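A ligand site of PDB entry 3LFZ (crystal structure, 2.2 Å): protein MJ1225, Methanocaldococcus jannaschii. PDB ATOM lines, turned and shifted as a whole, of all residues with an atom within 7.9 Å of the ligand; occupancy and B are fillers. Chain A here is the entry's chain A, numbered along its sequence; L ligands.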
ATOM      1  N   ILE A  23      -5.742 -29.916 -13.108  1.00  0.00           N
ATOM      2  CA  ILE A  23      -4.346 -30.322 -12.971  1.00  0.00           C
ATOM      3  C   ILE A  23      -4.190 -31.820 -13.268  1.00  0.00           C
ATOM      4  O   ILE A  23      -3.274 -32.211 -13.999  1.00  0.00           O
ATOM      5  CB  ILE A  23      -3.772 -29.956 -11.584  1.00  0.00           C
ATOM      6  CG1 ILE A  23      -3.800 -28.426 -11.384  1.00  0.00           C
ATOM      7  CG2 ILE A  23      -2.342 -30.499 -11.427  1.00  0.00           C
ATOM      8  CD1 ILE A  23      -3.579 -27.955  -9.946  1.00  0.00           C
ATOM      9  N   ASP A  59       6.911 -27.985  -8.745  1.00  0.00           N
ATOM     10  CA  ASP A  59       6.676 -26.866  -7.837  1.00  0.00           C
ATOM     11  C   ASP A  59       5.491 -27.201  -6.908  1.00  0.00           C
ATOM     12  O   ASP A  59       5.617 -27.222  -5.681  1.00  0.00           O
ATOM     13  CB  ASP A  59       6.384 -25.609  -8.672  1.00  0.00           C
ATOM     14  CG  ASP A  59       6.389 -24.316  -7.867  1.00  0.00           C
ATOM     15  OD1 ASP A  59       5.910 -24.287  -6.719  1.00  0.00           O
ATOM     16  OD2 ASP A  59       6.862 -23.291  -8.405  1.00  0.00           O
ATOM     17  N   PHE A  60       4.346 -27.456  -7.539  1.00  0.00           N
ATOM     18  CA  PHE A  60       3.093 -27.914  -6.939  1.00  0.00           C
ATOM     19  C   PHE A  60       3.248 -29.114  -5.978  1.00  0.00           C
ATOM     20  O   PHE A  60       2.604 -29.150  -4.933  1.00  0.00           O
ATOM     21  CB  PHE A  60       2.134 -28.215  -8.095  1.00  0.00           C
ATOM     22  CG  PHE A  60       0.844 -28.895  -7.710  1.00  0.00           C
ATOM     23  CD1 PHE A  60      -0.186 -28.182  -7.101  1.00  0.00           C
ATOM     24  CD2 PHE A  60       0.641 -30.227  -8.037  1.00  0.00           C
ATOM     25  CE1 PHE A  60      -1.386 -28.812  -6.785  1.00  0.00           C
ATOM     26  CE2 PHE A  60      -0.558 -30.860  -7.734  1.00  0.00           C
ATOM     27  CZ  PHE A  60      -1.573 -30.162  -7.113  1.00  0.00           C
ATOM     28  N   GLY A  64       8.194 -25.694  -4.602  1.00  0.00           N
ATOM     29  CA  GLY A  64       8.059 -24.246  -4.525  1.00  0.00           C
ATOM     30  C   GLY A  64       6.731 -23.775  -3.970  1.00  0.00           C
ATOM     31  O   GLY A  64       6.037 -24.527  -3.284  1.00  0.00           O
ATOM     32  N   SER A  65       6.381 -22.541  -4.295  1.00  0.00           N
ATOM     33  CA  SER A  65       5.227 -21.868  -3.711  1.00  0.00           C
ATOM     34  C   SER A  65       3.878 -22.474  -4.114  1.00  0.00           C
ATOM     35  O   SER A  65       2.884 -22.292  -3.409  1.00  0.00           O
ATOM     36  CB  SER A  65       5.264 -20.368  -4.029  1.00  0.00           C
ATOM     37  OG  SER A  65       4.214 -19.666  -3.376  1.00  0.00           O
ATOM     38  N   LYS A  66       3.839 -23.200  -5.227  1.00  0.00           N
ATOM     39  CA  LYS A  66       2.583 -23.797  -5.711  1.00  0.00           C
ATOM     40  C   LYS A  66       2.099 -24.970  -4.848  1.00  0.00           C
ATOM     41  O   LYS A  66       0.924 -25.332  -4.882  1.00  0.00           O
ATOM     42  CB  LYS A  66       2.700 -24.170  -7.195  1.00  0.00           C
ATOM     43  CG  LYS A  66       2.812 -22.952  -8.097  1.00  0.00           C
ATOM     44  CD  LYS A  66       3.249 -23.280  -9.517  1.00  0.00           C
ATOM     45  CE  LYS A  66       3.714 -21.999 -10.209  1.00  0.00           C
ATOM     46  NZ  LYS A  66       3.756 -22.119 -11.686  1.00  0.00           N
ATOM     47  N   TYR A  67       3.023 -25.521  -4.062  1.00  0.00           N
ATOM     48  CA  TYR A  67       2.731 -26.582  -3.097  1.00  0.00           C
ATOM     49  C   TYR A  67       1.650 -26.223  -2.077  1.00  0.00           C
ATOM     50  O   TYR A  67       0.941 -27.106  -1.580  1.00  0.00           O
ATOM     51  CB  TYR A  67       4.009 -26.990  -2.381  1.00  0.00           C
ATOM     52  CG  TYR A  67       3.842 -28.083  -1.338  1.00  0.00           C
ATOM     53  CD1 TYR A  67       3.265 -29.307  -1.669  1.00  0.00           C
ATOM     54  CD2 TYR A  67       4.296 -27.892  -0.032  1.00  0.00           C
ATOM     55  CE1 TYR A  67       3.122 -30.308  -0.717  1.00  0.00           C
ATOM     56  CE2 TYR A  67       4.153 -28.893   0.919  1.00  0.00           C
ATOM     57  CZ  TYR A  67       3.571 -30.099   0.577  1.00  0.00           C
ATOM     58  OH  TYR A  67       3.425 -31.090   1.511  1.00  0.00           O
ATOM     59  N   ASN A  68       1.540 -24.929  -1.765  1.00  0.00           N
ATOM     60  CA  ASN A  68       0.556 -24.478  -0.778  1.00  0.00           C
ATOM     61  C   ASN A  68      -0.897 -24.609  -1.227  1.00  0.00           C
ATOM     62  O   ASN A  68      -1.815 -24.504  -0.417  1.00  0.00           O
ATOM     63  CB  ASN A  68       0.865 -23.062  -0.292  1.00  0.00           C
ATOM     64  CG  ASN A  68       1.730 -23.056   0.966  1.00  0.00           C
ATOM     65  OD1 ASN A  68       2.470 -24.004   1.228  1.00  0.00           O
ATOM     66  ND2 ASN A  68       1.619 -21.984   1.744  1.00  0.00           N
ATOM     67  N   LEU A  69      -1.102 -24.854  -2.525  1.00  0.00           N
ATOM     68  CA  LEU A  69      -2.415 -25.246  -3.032  1.00  0.00           C
ATOM     69  C   LEU A  69      -2.816 -26.589  -2.422  1.00  0.00           C
ATOM     70  O   LEU A  69      -3.964 -26.779  -2.011  1.00  0.00           O
ATOM     71  CB  LEU A  69      -2.418 -25.319  -4.568  1.00  0.00           C
ATOM     72  CG  LEU A  69      -3.734 -25.589  -5.308  1.00  0.00           C
ATOM     73  CD1 LEU A  69      -4.800 -24.526  -5.016  1.00  0.00           C
ATOM     74  CD2 LEU A  69      -3.498 -25.719  -6.800  1.00  0.00           C
ATOM     75  N   ILE A  70      -1.858 -27.509  -2.356  1.00  0.00           N
ATOM     76  CA  ILE A  70      -2.045 -28.775  -1.633  1.00  0.00           C
ATOM     77  C   ILE A  70      -2.052 -28.542  -0.120  1.00  0.00           C
ATOM     78  O   ILE A  70      -3.078 -28.768   0.530  1.00  0.00           O
ATOM     79  CB  ILE A  70      -0.959 -29.829  -2.005  1.00  0.00           C
ATOM     80  CG1 ILE A  70      -0.964 -30.123  -3.505  1.00  0.00           C
ATOM     81  CG2 ILE A  70      -1.151 -31.119  -1.189  1.00  0.00           C
ATOM     82  CD1 ILE A  70       0.218 -30.952  -3.985  1.00  0.00           C
ATOM     83  N   ARG A  71      -0.927 -28.065   0.422  1.00  0.00           N
ATOM     84  CA  ARG A  71      -0.724 -27.985   1.881  1.00  0.00           C
ATOM     85  C   ARG A  71      -1.775 -27.122   2.592  1.00  0.00           C
ATOM     86  O   ARG A  71      -2.309 -27.523   3.630  1.00  0.00           O
ATOM     87  CB  ARG A  71       0.726 -27.583   2.254  1.00  0.00           C
ATOM     88  CG  ARG A  71       1.137 -27.908   3.725  1.00  0.00           C
ATOM     89  CD  ARG A  71       2.665 -27.925   3.982  1.00  0.00           C
ATOM     90  NE  ARG A  71       3.215 -29.280   4.180  1.00  0.00           N
ATOM     91  CZ  ARG A  71       4.468 -29.555   4.557  1.00  0.00           C
ATOM     92  NH1 ARG A  71       5.340 -28.578   4.777  1.00  0.00           N
ATOM     93  NH2 ARG A  71       4.861 -30.813   4.709  1.00  0.00           N
ATOM     94  N   GLU A  72      -2.105 -25.961   2.024  1.00  0.00           N
ATOM     95  CA  GLU A  72      -3.032 -25.024   2.686  1.00  0.00           C
ATOM     96  C   GLU A  72      -4.499 -25.180   2.307  1.00  0.00           C
ATOM     97  O   GLU A  72      -5.296 -25.664   3.118  1.00  0.00           O
ATOM     98  CB  GLU A  72      -2.573 -23.570   2.515  1.00  0.00           C
ATOM     99  CG  GLU A  72      -1.373 -23.179   3.368  1.00  0.00           C
ATOM    100  CD  GLU A  72      -1.567 -23.492   4.842  1.00  0.00           C
ATOM    101  OE1 GLU A  72      -2.616 -23.133   5.413  1.00  0.00           O
ATOM    102  OE2 GLU A  72      -0.653 -24.097   5.436  1.00  0.00           O
ATOM    103  N   LYS A  73      -4.874 -24.761   1.095  1.00  0.00           N
ATOM    104  CA  LYS A  73      -6.274 -24.800   0.666  1.00  0.00           C
ATOM    105  C   LYS A  73      -6.889 -26.194   0.793  1.00  0.00           C
ATOM    106  O   LYS A  73      -8.053 -26.335   1.176  1.00  0.00           O
ATOM    107  CB  LYS A  73      -6.413 -24.279  -0.772  1.00  0.00           C
ATOM    108  CG  LYS A  73      -7.861 -24.078  -1.217  1.00  0.00           C
ATOM    109  CD  LYS A  73      -7.947 -23.344  -2.552  1.00  0.00           C
ATOM    110  CE  LYS A  73      -9.402 -23.126  -2.951  1.00  0.00           C
ATOM    111  NZ  LYS A  73      -9.507 -22.369  -4.235  1.00  0.00           N
ATOM    112  N   HIS A  74      -6.088 -27.221   0.496  1.00  0.00           N
ATOM    113  CA  HIS A  74      -6.577 -28.602   0.458  1.00  0.00           C
ATOM    114  C   HIS A  74      -5.988 -29.501   1.531  1.00  0.00           C
ATOM    115  O   HIS A  74      -6.083 -30.732   1.454  1.00  0.00           O
ATOM    116  CB  HIS A  74      -6.370 -29.194  -0.924  1.00  0.00           C
ATOM    117  CG  HIS A  74      -7.208 -28.532  -1.975  1.00  0.00           C
ATOM    118  ND1 HIS A  74      -8.477 -28.973  -2.284  1.00  0.00           N
ATOM    119  CD2 HIS A  74      -6.977 -27.458  -2.759  1.00  0.00           C
ATOM    120  CE1 HIS A  74      -8.985 -28.204  -3.225  1.00  0.00           C
ATOM    121  NE2 HIS A  74      -8.096 -27.272  -3.525  1.00  0.00           N
ATOM    122  N   GLU A  75      -5.384 -28.880   2.535  1.00  0.00           N
ATOM    123  CA  GLU A  75      -4.955 -29.562   3.761  1.00  0.00           C
ATOM    124  C   GLU A  75      -4.274 -30.895   3.471  1.00  0.00           C
ATOM    125  O   GLU A  75      -4.711 -31.958   3.934  1.00  0.00           O
ATOM    126  CB  GLU A  75      -6.135 -29.662   4.731  1.00  0.00           C
ATOM    127  CG  GLU A  75      -6.508 -28.294   5.328  1.00  0.00           C
ATOM    128  CD  GLU A  75      -8.004 -28.048   5.408  1.00  0.00           C
ATOM    129  OE1 GLU A  75      -8.715 -28.870   6.021  1.00  0.00           O
ATOM    130  OE2 GLU A  75      -8.468 -27.023   4.864  1.00  0.00           O
ATOM    131  N   GLU A  84      -8.307 -29.016  -8.992  1.00  0.00           N
ATOM    132  CA  GLU A  84      -8.221 -27.576  -9.248  1.00  0.00           C
ATOM    133  C   GLU A  84      -7.942 -27.328 -10.727  1.00  0.00           C
ATOM    134  O   GLU A  84      -7.209 -28.096 -11.353  1.00  0.00           O
ATOM    135  CB  GLU A  84      -7.127 -26.932  -8.383  1.00  0.00           C
ATOM    136  CG  GLU A  84      -7.465 -26.813  -6.891  1.00  0.00           C
ATOM    137  CD  GLU A  84      -8.352 -25.622  -6.567  1.00  0.00           C
ATOM    138  OE1 GLU A  84      -8.778 -25.501  -5.398  1.00  0.00           O
ATOM    139  OE2 GLU A  84      -8.638 -24.793  -7.464  1.00  0.00           O
ATOM    140  N   PRO A  85      -8.518 -26.254 -11.293  1.00  0.00           N
ATOM    141  CA  PRO A  85      -8.221 -25.940 -12.691  1.00  0.00           C
ATOM    142  C   PRO A  85      -6.739 -25.598 -12.848  1.00  0.00           C
ATOM    143  O   PRO A  85      -6.107 -25.089 -11.926  1.00  0.00           O
ATOM    144  CB  PRO A  85      -9.086 -24.711 -12.979  1.00  0.00           C
ATOM    145  CG  PRO A  85      -9.324 -24.087 -11.644  1.00  0.00           C
ATOM    146  CD  PRO A  85      -9.408 -25.234 -10.682  1.00  0.00           C
ATOM    147  N   ARG A  87      -5.332 -23.289 -14.331  1.00  0.00           N
ATOM    148  CA  ARG A  87      -5.071 -21.859 -14.225  1.00  0.00           C
ATOM    149  C   ARG A  87      -4.516 -21.470 -12.845  1.00  0.00           C
ATOM    150  O   ARG A  87      -3.897 -20.424 -12.695  1.00  0.00           O
ATOM    151  CB  ARG A  87      -6.326 -21.041 -14.544  1.00  0.00           C
ATOM    152  CG  ARG A  87      -7.383 -21.044 -13.446  1.00  0.00           C
ATOM    153  CD  ARG A  87      -8.691 -20.466 -13.942  1.00  0.00           C
ATOM    154  NE  ARG A  87      -9.755 -20.665 -12.967  1.00  0.00           N
ATOM    155  CZ  ARG A  87     -11.049 -20.713 -13.266  1.00  0.00           C
ATOM    156  NH1 ARG A  87     -11.450 -20.591 -14.529  1.00  0.00           N
ATOM    157  NH2 ARG A  87     -11.945 -20.907 -12.305  1.00  0.00           N
ATOM    158  N   GLU A  88      -4.725 -22.336 -11.851  1.00  0.00           N
ATOM    159  CA  GLU A  88      -4.227 -22.092 -10.487  1.00  0.00           C
ATOM    160  C   GLU A  88      -2.714 -22.244 -10.375  1.00  0.00           C
ATOM    161  O   GLU A  88      -2.098 -21.654  -9.473  1.00  0.00           O
ATOM    162  CB  GLU A  88      -4.924 -23.014  -9.478  1.00  0.00           C
ATOM    163  CG  GLU A  88      -6.393 -22.672  -9.185  1.00  0.00           C
ATOM    164  CD  GLU A  88      -6.567 -21.414  -8.346  1.00  0.00           C
ATOM    165  OE1 GLU A  88      -5.652 -21.050  -7.566  1.00  0.00           O
ATOM    166  OE2 GLU A  88      -7.641 -20.774  -8.461  1.00  0.00           O
ATOM    167  N   ILE A  89      -2.108 -23.023 -11.266  1.00  0.00           N
ATOM    168  CA  ILE A  89      -0.666 -23.275 -11.211  1.00  0.00           C
ATOM    169  C   ILE A  89       0.096 -23.002 -12.524  1.00  0.00           C
ATOM    170  O   ILE A  89       1.321 -23.166 -12.569  1.00  0.00           O
ATOM    171  CB  ILE A  89      -0.324 -24.722 -10.692  1.00  0.00           C
ATOM    172  CG1 ILE A  89      -0.854 -25.789 -11.652  1.00  0.00           C
ATOM    173  CG2 ILE A  89      -0.847 -24.928  -9.276  1.00  0.00           C
ATOM    174  CD1 ILE A  89      -0.181 -27.163 -11.474  1.00  0.00           C
ATOM    175  N   MET A  90      -0.616 -22.596 -13.570  1.00  0.00           N
ATOM    176  CA  MET A  90       0.057 -22.310 -14.837  1.00  0.00           C
ATOM    177  C   MET A  90       0.855 -21.006 -14.743  1.00  0.00           C
ATOM    178  O   MET A  90       0.559 -20.142 -13.914  1.00  0.00           O
ATOM    179  CB  MET A  90      -0.953 -22.235 -15.989  1.00  0.00           C
ATOM    180  CG  MET A  90      -1.803 -20.976 -16.005  1.00  0.00           C
ATOM    181  SD  MET A  90      -3.058 -21.009 -17.296  1.00  0.00           S
ATOM    182  CE  MET A  90      -3.829 -19.402 -17.077  1.00  0.00           C
HETATM  183  P1  LIG L   1      -8.034 -19.618  -0.325  1.00  0.00           P
HETATM  184  O1  LIG L   1      -8.116 -18.150  -0.094  1.00  0.00           O
HETATM  185  O2  LIG L   1      -8.446 -20.018  -1.841  1.00  0.00           O
HETATM  186  O3  LIG L   1      -9.073 -20.430   0.618  1.00  0.00           O
HETATM  187  O4  LIG L   1      -6.583 -20.260  -0.078  1.00  0.00           O
HETATM  188  C1  LIG L   1      -6.126 -20.556   1.238  1.00  0.00           C
HETATM  189  C2  LIG L   1      -4.622 -20.735   1.232  1.00  0.00           C
HETATM  190  O5  LIG L   1      -4.299 -21.768   0.276  1.00  0.00           O
HETATM  191  C3  LIG L   1      -3.977 -19.466   0.677  1.00  0.00           C
HETATM  192  O6  LIG L   1      -3.688 -18.569   1.754  1.00  0.00           O
HETATM  193  C4  LIG L   1      -2.693 -19.990   0.065  1.00  0.00           C
HETATM  194  O7  LIG L   1      -1.678 -20.131   1.072  1.00  0.00           O
HETATM  195  C5  LIG L   1      -3.085 -21.375  -0.437  1.00  0.00           C
HETATM  196  N1  LIG L   1      -3.326 -21.340  -1.905  1.00  0.00           N
HETATM  197  C6  LIG L   1      -4.507 -21.234  -2.520  1.00  0.00           C
HETATM  198  N2  LIG L   1      -4.303 -21.246  -3.845  1.00  0.00           N
HETATM  199  C7  LIG L   1      -3.005 -21.362  -4.061  1.00  0.00           C
HETATM  200  C8  LIG L   1      -2.207 -21.432  -5.205  1.00  0.00           C
HETATM  201  N3  LIG L   1      -2.759 -21.370  -6.418  1.00  0.00           N
HETATM  202  N4  LIG L   1      -0.875 -21.552  -5.067  1.00  0.00           N
HETATM  203  C9  LIG L   1      -0.314 -21.609  -3.876  1.00  0.00           C
HETATM  204  N5  LIG L   1      -1.045 -21.548  -2.760  1.00  0.00           N
HETATM  205  C10 LIG L   1      -2.382 -21.421  -2.834  1.00  0.00           C
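The backbone carbonyl oxygen (O) of Glu 88 sits at hydrogen-bond distance from a nitrogen (N3) of the ligand (3.1 Å).
OE1 of Glu 88 lies within hydrogen-bond range of N3 of the ligand (3.1 Å).
N of Lys 73 is in hydrogen-bond range of O5 of the ligand.
An oxygen (O2) of the ligand lies within salt-bridge range of the side-chain amino group of Lys 73 (3.5 Å).
The backbone NH (N) of Leu 69 is in hydrogen-bond range of a nitrogen (N5) of the ligand (3.3 Å).
Merely in contact with the ligand: Ser 65 (3.3 Å), Asn 68 (3.4 Å) and Glu 72 (3.4 Å).
Hydrophobic or aromatic side chains that line the ligand: Leu 69.
Of the 21 residues printed, 6 come within 4 Å of the ligand.
The nearest printed residue that does not touch the ligand is Lys 66 (4.1 Å).
The backbone NH (N) of Lys 73 lies within hydrogen-bond range of the backbone carbonyl oxygen (O) of Asn 68, at 3.4 Å.
OE1 of Glu 84 is in salt-bridge range of NZ of Lys 73, 3.4 Å away.
N of Ser 65 sits at hydrogen-bond distance from OD1 of Asp 59 (3.0 Å).
O of Leu 69 lies close to N of His 74 (3.3 Å).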
